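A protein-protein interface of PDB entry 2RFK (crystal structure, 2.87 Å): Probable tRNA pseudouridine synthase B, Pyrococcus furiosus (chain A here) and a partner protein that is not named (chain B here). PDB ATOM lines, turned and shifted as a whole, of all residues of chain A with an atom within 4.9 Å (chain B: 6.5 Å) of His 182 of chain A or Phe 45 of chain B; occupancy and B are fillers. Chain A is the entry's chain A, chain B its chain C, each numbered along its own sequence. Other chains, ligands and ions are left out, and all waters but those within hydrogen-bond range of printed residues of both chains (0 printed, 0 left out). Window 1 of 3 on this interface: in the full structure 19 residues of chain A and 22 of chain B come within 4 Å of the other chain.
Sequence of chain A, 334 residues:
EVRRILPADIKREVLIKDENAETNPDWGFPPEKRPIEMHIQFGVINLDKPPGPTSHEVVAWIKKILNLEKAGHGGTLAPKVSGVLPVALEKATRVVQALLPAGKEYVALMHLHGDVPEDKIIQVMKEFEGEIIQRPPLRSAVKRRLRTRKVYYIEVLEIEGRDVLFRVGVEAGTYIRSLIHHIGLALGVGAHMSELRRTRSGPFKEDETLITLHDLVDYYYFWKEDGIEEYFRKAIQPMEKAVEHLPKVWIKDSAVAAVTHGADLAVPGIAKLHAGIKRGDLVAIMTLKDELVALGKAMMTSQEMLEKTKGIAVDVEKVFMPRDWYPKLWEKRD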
ATOM      1  N   PHE A 128       0.793  -3.760  24.551  1.00  0.00           N
ATOM      2  CA  PHE A 128       1.120  -3.674  23.124  1.00  0.00           C
ATOM      3  C   PHE A 128       1.793  -4.930  22.521  1.00  0.00           C
ATOM      4  O   PHE A 128       2.351  -4.883  21.418  1.00  0.00           O
ATOM      5  CB  PHE A 128       1.986  -2.442  22.861  1.00  0.00           C
ATOM      6  CG  PHE A 128       1.202  -1.206  22.561  1.00  0.00           C
ATOM      7  CD1 PHE A 128       0.737  -0.960  21.273  1.00  0.00           C
ATOM      8  CD2 PHE A 128       0.932  -0.281  23.559  1.00  0.00           C
ATOM      9  CE1 PHE A 128       0.009   0.187  20.982  1.00  0.00           C
ATOM     10  CE2 PHE A 128       0.205   0.870  23.278  1.00  0.00           C
ATOM     11  CZ  PHE A 128      -0.259   1.103  21.985  1.00  0.00           C
ATOM     12  N   ILE A 133      -3.664  -2.803  16.388  1.00  0.00           N
ATOM     13  CA  ILE A 133      -4.327  -1.973  15.384  1.00  0.00           C
ATOM     14  C   ILE A 133      -3.369  -0.940  14.798  1.00  0.00           C
ATOM     15  O   ILE A 133      -2.698  -0.231  15.546  1.00  0.00           O
ATOM     16  CB  ILE A 133      -5.529  -1.248  16.023  1.00  0.00           C
ATOM     17  CG1 ILE A 133      -6.673  -2.238  16.249  1.00  0.00           C
ATOM     18  CG2 ILE A 133      -5.985  -0.080  15.157  1.00  0.00           C
ATOM     19  CD1 ILE A 133      -7.606  -1.867  17.368  1.00  0.00           C
ATOM     20  N   SER A 178       5.763   5.676  14.335  1.00  0.00           N
ATOM     21  CA  SER A 178       4.325   5.553  14.494  1.00  0.00           C
ATOM     22  C   SER A 178       3.902   4.783  15.743  1.00  0.00           C
ATOM     23  O   SER A 178       2.824   5.046  16.294  1.00  0.00           O
ATOM     24  CB  SER A 178       3.719   4.895  13.240  1.00  0.00           C
ATOM     25  OG  SER A 178       2.350   4.548  13.418  1.00  0.00           O
ATOM     26  N   LEU A 179       4.723   3.834  16.180  1.00  0.00           N
ATOM     27  CA  LEU A 179       4.351   3.025  17.334  1.00  0.00           C
ATOM     28  C   LEU A 179       4.622   3.736  18.652  1.00  0.00           C
ATOM     29  O   LEU A 179       3.787   3.718  19.559  1.00  0.00           O
ATOM     30  CB  LEU A 179       5.050   1.666  17.304  1.00  0.00           C
ATOM     31  CG  LEU A 179       4.757   0.725  18.482  1.00  0.00           C
ATOM     32  CD1 LEU A 179       3.254   0.466  18.672  1.00  0.00           C
ATOM     33  CD2 LEU A 179       5.512  -0.576  18.315  1.00  0.00           C
ATOM     34  N   ILE A 180       5.800   4.347  18.750  1.00  0.00           N
ATOM     35  CA  ILE A 180       6.226   5.056  19.947  1.00  0.00           C
ATOM     36  C   ILE A 180       5.262   6.201  20.223  1.00  0.00           C
ATOM     37  O   ILE A 180       4.713   6.340  21.322  1.00  0.00           O
ATOM     38  CB  ILE A 180       7.662   5.558  19.772  1.00  0.00           C
ATOM     39  CG1 ILE A 180       8.632   4.373  19.906  1.00  0.00           C
ATOM     40  CG2 ILE A 180       7.980   6.623  20.779  1.00  0.00           C
ATOM     41  CD1 ILE A 180      10.015   4.564  19.246  1.00  0.00           C
ATOM     42  N   HIS A 181       5.048   6.994  19.185  1.00  0.00           N
ATOM     43  CA  HIS A 181       4.109   8.089  19.204  1.00  0.00           C
ATOM     44  C   HIS A 181       2.726   7.678  19.738  1.00  0.00           C
ATOM     45  O   HIS A 181       2.059   8.459  20.424  1.00  0.00           O
ATOM     46  CB  HIS A 181       4.009   8.634  17.788  1.00  0.00           C
ATOM     47  CG  HIS A 181       2.910   9.620  17.599  1.00  0.00           C
ATOM     48  ND1 HIS A 181       1.630   9.246  17.253  1.00  0.00           N
ATOM     49  CD2 HIS A 181       2.896  10.967  17.713  1.00  0.00           C
ATOM     50  CE1 HIS A 181       0.874  10.323  17.157  1.00  0.00           C
ATOM     51  NE2 HIS A 181       1.618  11.379  17.431  1.00  0.00           N
ATOM     52  N   HIS A 182       2.311   6.455  19.426  1.00  0.00           N
ATOM     53  CA  HIS A 182       1.003   5.930  19.833  1.00  0.00           C
ATOM     54  C   HIS A 182       0.961   5.539  21.298  1.00  0.00           C
ATOM     55  O   HIS A 182      -0.002   5.832  21.986  1.00  0.00           O
ATOM     56  CB  HIS A 182       0.605   4.732  18.971  1.00  0.00           C
ATOM     57  CG  HIS A 182      -0.027   5.109  17.668  1.00  0.00           C
ATOM     58  ND1 HIS A 182       0.295   6.264  16.989  1.00  0.00           N
ATOM     59  CD2 HIS A 182      -0.950   4.472  16.909  1.00  0.00           C
ATOM     60  CE1 HIS A 182      -0.408   6.327  15.871  1.00  0.00           C
ATOM     61  NE2 HIS A 182      -1.174   5.252  15.802  1.00  0.00           N
ATOM     62  N   ILE A 183       2.001   4.866  21.768  1.00  0.00           N
ATOM     63  CA  ILE A 183       2.161   4.591  23.196  1.00  0.00           C
ATOM     64  C   ILE A 183       2.305   5.925  23.946  1.00  0.00           C
ATOM     65  O   ILE A 183       1.800   6.087  25.067  1.00  0.00           O
ATOM     66  CB  ILE A 183       3.327   3.553  23.480  1.00  0.00           C
ATOM     67  CG1 ILE A 183       4.058   3.836  24.798  1.00  0.00           C
ATOM     68  CG2 ILE A 183       4.317   3.469  22.334  1.00  0.00           C
ATOM     69  CD1 ILE A 183       3.598   2.953  25.948  1.00  0.00           C
ATOM     70  N   GLY A 184       2.968   6.879  23.293  1.00  0.00           N
ATOM     71  CA  GLY A 184       3.045   8.253  23.782  1.00  0.00           C
ATOM     72  C   GLY A 184       1.661   8.772  24.079  1.00  0.00           C
ATOM     73  O   GLY A 184       1.336   9.046  25.233  1.00  0.00           O
ATOM     74  N   LEU A 185       0.844   8.874  23.034  1.00  0.00           N
ATOM     75  CA  LEU A 185      -0.565   9.246  23.165  1.00  0.00           C
ATOM     76  C   LEU A 185      -1.234   8.492  24.300  1.00  0.00           C
ATOM     77  O   LEU A 185      -1.975   9.077  25.080  1.00  0.00           O
ATOM     78  CB  LEU A 185      -1.321   8.956  21.861  1.00  0.00           C
ATOM     79  CG  LEU A 185      -1.616  10.014  20.790  1.00  0.00           C
ATOM     80  CD1 LEU A 185      -0.418  10.896  20.486  1.00  0.00           C
ATOM     81  CD2 LEU A 185      -2.140   9.358  19.499  1.00  0.00           C
ATOM     82  N   ALA A 186      -0.957   7.194  24.391  1.00  0.00           N
ATOM     83  CA  ALA A 186      -1.661   6.300  25.315  1.00  0.00           C
ATOM     84  C   ALA A 186      -1.283   6.529  26.763  1.00  0.00           C
ATOM     85  O   ALA A 186      -2.112   6.384  27.659  1.00  0.00           O
ATOM     86  CB  ALA A 186      -1.437   4.849  24.938  1.00  0.00           C
ATOM     87  N   ILE B  17      -8.379  10.339  26.225  1.00  0.00           N
ATOM     88  CA  ILE B  17      -8.116   8.909  26.087  1.00  0.00           C
ATOM     89  C   ILE B  17      -9.139   8.074  26.843  1.00  0.00           C
ATOM     90  O   ILE B  17      -9.064   7.925  28.067  1.00  0.00           O
ATOM     91  CB  ILE B  17      -6.694   8.498  26.531  1.00  0.00           C
ATOM     92  CG1 ILE B  17      -5.633   9.416  25.923  1.00  0.00           C
ATOM     93  CG2 ILE B  17      -6.429   7.059  26.146  1.00  0.00           C
ATOM     94  CD1 ILE B  17      -5.152  10.477  26.875  1.00  0.00           C
ATOM     95  N   ASP B  43      -7.721   8.402  16.140  1.00  0.00           N
ATOM     96  CA  ASP B  43      -6.937   7.170  16.232  1.00  0.00           C
ATOM     97  C   ASP B  43      -7.573   6.135  17.153  1.00  0.00           C
ATOM     98  O   ASP B  43      -8.051   6.445  18.250  1.00  0.00           O
ATOM     99  CB  ASP B  43      -5.493   7.468  16.692  1.00  0.00           C
ATOM    100  CG  ASP B  43      -4.415   6.750  15.845  1.00  0.00           C
ATOM    101  OD1 ASP B  43      -3.278   7.271  15.780  1.00  0.00           O
ATOM    102  OD2 ASP B  43      -4.687   5.684  15.248  1.00  0.00           O
ATOM    103  N   VAL B  44      -7.602   4.908  16.653  1.00  0.00           N
ATOM    104  CA  VAL B  44      -7.638   3.727  17.492  1.00  0.00           C
ATOM    105  C   VAL B  44      -6.296   3.067  17.224  1.00  0.00           C
ATOM    106  O   VAL B  44      -5.750   3.171  16.118  1.00  0.00           O
ATOM    107  CB  VAL B  44      -8.818   2.792  17.166  1.00  0.00           C
ATOM    108  CG1 VAL B  44      -8.849   1.594  18.112  1.00  0.00           C
ATOM    109  CG2 VAL B  44     -10.119   3.555  17.272  1.00  0.00           C
ATOM    110  N   PHE B  45      -5.749   2.418  18.244  1.00  0.00           N
ATOM    111  CA  PHE B  45      -4.371   1.930  18.213  1.00  0.00           C
ATOM    112  C   PHE B  45      -4.128   0.994  19.388  1.00  0.00           C
ATOM    113  O   PHE B  45      -4.528   1.280  20.514  1.00  0.00           O
ATOM    114  CB  PHE B  45      -3.403   3.118  18.292  1.00  0.00           C
ATOM    115  CG  PHE B  45      -3.690   4.068  19.436  1.00  0.00           C
ATOM    116  CD1 PHE B  45      -4.858   4.845  19.453  1.00  0.00           C
ATOM    117  CD2 PHE B  45      -2.798   4.187  20.499  1.00  0.00           C
ATOM    118  CE1 PHE B  45      -5.135   5.715  20.507  1.00  0.00           C
ATOM    119  CE2 PHE B  45      -3.063   5.060  21.561  1.00  0.00           C
ATOM    120  CZ  PHE B  45      -4.235   5.833  21.561  1.00  0.00           C
ATOM    121  N   GLY B  46      -3.467  -0.123  19.133  1.00  0.00           N
ATOM    122  CA  GLY B  46      -3.183  -1.070  20.205  1.00  0.00           C
ATOM    123  C   GLY B  46      -4.160  -2.228  20.250  1.00  0.00           C
ATOM    124  O   GLY B  46      -5.139  -2.235  19.496  1.00  0.00           O
ATOM    125  N   PRO B  47      -3.928  -3.180  21.181  1.00  0.00           N
ATOM    126  CA  PRO B  47      -4.412  -4.559  21.145  1.00  0.00           C
ATOM    127  C   PRO B  47      -5.826  -4.673  20.585  1.00  0.00           C
ATOM    128  O   PRO B  47      -6.763  -4.115  21.159  1.00  0.00           O
ATOM    129  CB  PRO B  47      -4.353  -4.998  22.622  1.00  0.00           C
ATOM    130  CG  PRO B  47      -3.955  -3.775  23.399  1.00  0.00           C
ATOM    131  CD  PRO B  47      -3.209  -2.920  22.434  1.00  0.00           C
ATOM    132  N   MET B  50      -8.706  -5.196  23.223  1.00  0.00           N
ATOM    133  CA  MET B  50      -9.069  -4.046  24.071  1.00  0.00           C
ATOM    134  C   MET B  50      -8.249  -2.809  23.670  1.00  0.00           C
ATOM    135  O   MET B  50      -7.160  -2.579  24.219  1.00  0.00           O
ATOM    136  CB  MET B  50      -8.840  -4.364  25.555  1.00  0.00           C
ATOM    137  CG  MET B  50      -9.325  -5.743  26.005  1.00  0.00           C
ATOM    138  SD  MET B  50      -8.456  -6.367  27.468  1.00  0.00           S
ATOM    139  CE  MET B  50      -6.915  -7.026  26.779  1.00  0.00           C
ATOM    140  N   PRO B  51      -8.758  -2.022  22.696  1.00  0.00           N
ATOM    141  CA  PRO B  51      -7.975  -0.929  22.118  1.00  0.00           C
ATOM    142  C   PRO B  51      -7.868   0.345  22.964  1.00  0.00           C
ATOM    143  O   PRO B  51      -8.161   0.346  24.161  1.00  0.00           O
ATOM    144  CB  PRO B  51      -8.696  -0.640  20.784  1.00  0.00           C
ATOM    145  CG  PRO B  51      -9.776  -1.670  20.659  1.00  0.00           C
ATOM    146  CD  PRO B  51     -10.072  -2.135  22.043  1.00  0.00           C
ATOM    147  N   TYR B  52      -7.398   1.406  22.321  1.00  0.00           N
ATOM    148  CA  TYR B  52      -7.465   2.743  22.860  1.00  0.00           C
ATOM    149  C   TYR B  52      -8.130   3.643  21.820  1.00  0.00           C
ATOM    150  O   TYR B  52      -7.719   3.646  20.649  1.00  0.00           O
ATOM    151  CB  TYR B  52      -6.071   3.279  23.135  1.00  0.00           C
ATOM    152  CG  TYR B  52      -5.363   2.709  24.346  1.00  0.00           C
ATOM    153  CD1 TYR B  52      -5.714   3.099  25.639  1.00  0.00           C
ATOM    154  CD2 TYR B  52      -4.303   1.823  24.196  1.00  0.00           C
ATOM    155  CE1 TYR B  52      -5.043   2.594  26.754  1.00  0.00           C
ATOM    156  CE2 TYR B  52      -3.631   1.313  25.301  1.00  0.00           C
ATOM    157  CZ  TYR B  52      -4.002   1.701  26.575  1.00  0.00           C
ATOM    158  OH  TYR B  52      -3.323   1.196  27.665  1.00  0.00           O
ATOM    159  N   VAL B  53      -9.147   4.392  22.238  1.00  0.00           N
ATOM    160  CA  VAL B  53      -9.693   5.428  21.381  1.00  0.00           C
ATOM    161  C   VAL B  53      -9.095   6.764  21.785  1.00  0.00           C
ATOM    162  O   VAL B  53      -9.273   7.196  22.926  1.00  0.00           O
ATOM    163  CB  VAL B  53     -11.237   5.570  21.476  1.00  0.00           C
ATOM    164  CG1 VAL B  53     -11.766   6.073  20.162  1.00  0.00           C
ATOM    165  CG2 VAL B  53     -11.921   4.260  21.827  1.00  0.00           C
ATOM    166  N   ALA B  54      -8.393   7.421  20.863  1.00  0.00           N
ATOM    167  CA  ALA B  54      -7.899   8.785  21.112  1.00  0.00           C
ATOM    168  C   ALA B  54      -8.823   9.837  20.498  1.00  0.00           C
ATOM    169  O   ALA B  54      -9.115   9.789  19.297  1.00  0.00           O
ATOM    170  CB  ALA B  54      -6.492   8.954  20.595  1.00  0.00           C
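The backbone NH of Ile 133 of chain A lies close to the backbone carbonyl oxygen of Gly 46 of chain B, at 3.5 Å. NE2 of His 182 of chain A is in hydrogen-bond range of OD1 of Asp 43 of chain B, at 2.9 Å.
O of Ser 178 of chain A lies within hydrogen-bond range of ND1 of His 182 of chain A. ND1 of His 182 of chain A lies within hydrogen-bond range of ND1 of His 181 of chain A (3.3 Å). The backbone carbonyl oxygen (O) of Asp 43 of chain B sits at hydrogen-bond distance from the backbone NH (N) of Ala 54 of chain B, 2.8 Å away. The backbone NH (N) of Phe 45 of chain B sits close to the backbone carbonyl oxygen (O) of Tyr 52 of chain B (3.3 Å).
Among the printed residues, merely in contact across the chains: His 182 of chain A with Phe 45 of chain B, Ile 133 of chain A with Val 44 of chain B, Phe 128 of chain A with Gly 46 of chain B, Ala 186 of chain A with Phe 45 of chain B, Leu 185 of chain A with Ile 17 of chain B, Ile 133 of chain A with Pro 51 of chain B and Ile 133 of chain A with Phe 45 of chain B.
Of the printed residues of chain B, Phe 128 of chain A touches Gly 46 (3.5 Å). Ile 180 of chain A touches none of the printed residues of chain B. His 182 of chain A touches just these residues of chain B: Asp 43 and Phe 45. Printed residues of chain B within 4 Å of Leu 185 of chain A: Ile 17 (3.8 Å). Phe 45 of chain B touches three residues of chain A. Printed residues of chain A within 4 Å of Gly 46 of chain B: Phe 128 (3.5 Å) and Ile 133 (3.3 Å). Met 50 of chain B touches none of the printed residues of chain A. Of the printed residues of chain A, Pro 51 of chain B touches Ile 133 (3.8 Å). The nearest residue of chain B that does not touch His 182 of chain A is Val 44 of chain B (5.0 Å).
Printed residues of chain B that touch a printed residue of chain A: Ile 17, Asp 43, Val 44, Phe 45, Gly 46 and Pro 51. Of the 11 printed residues of chain A, 5 touch a printed residue of chain B.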
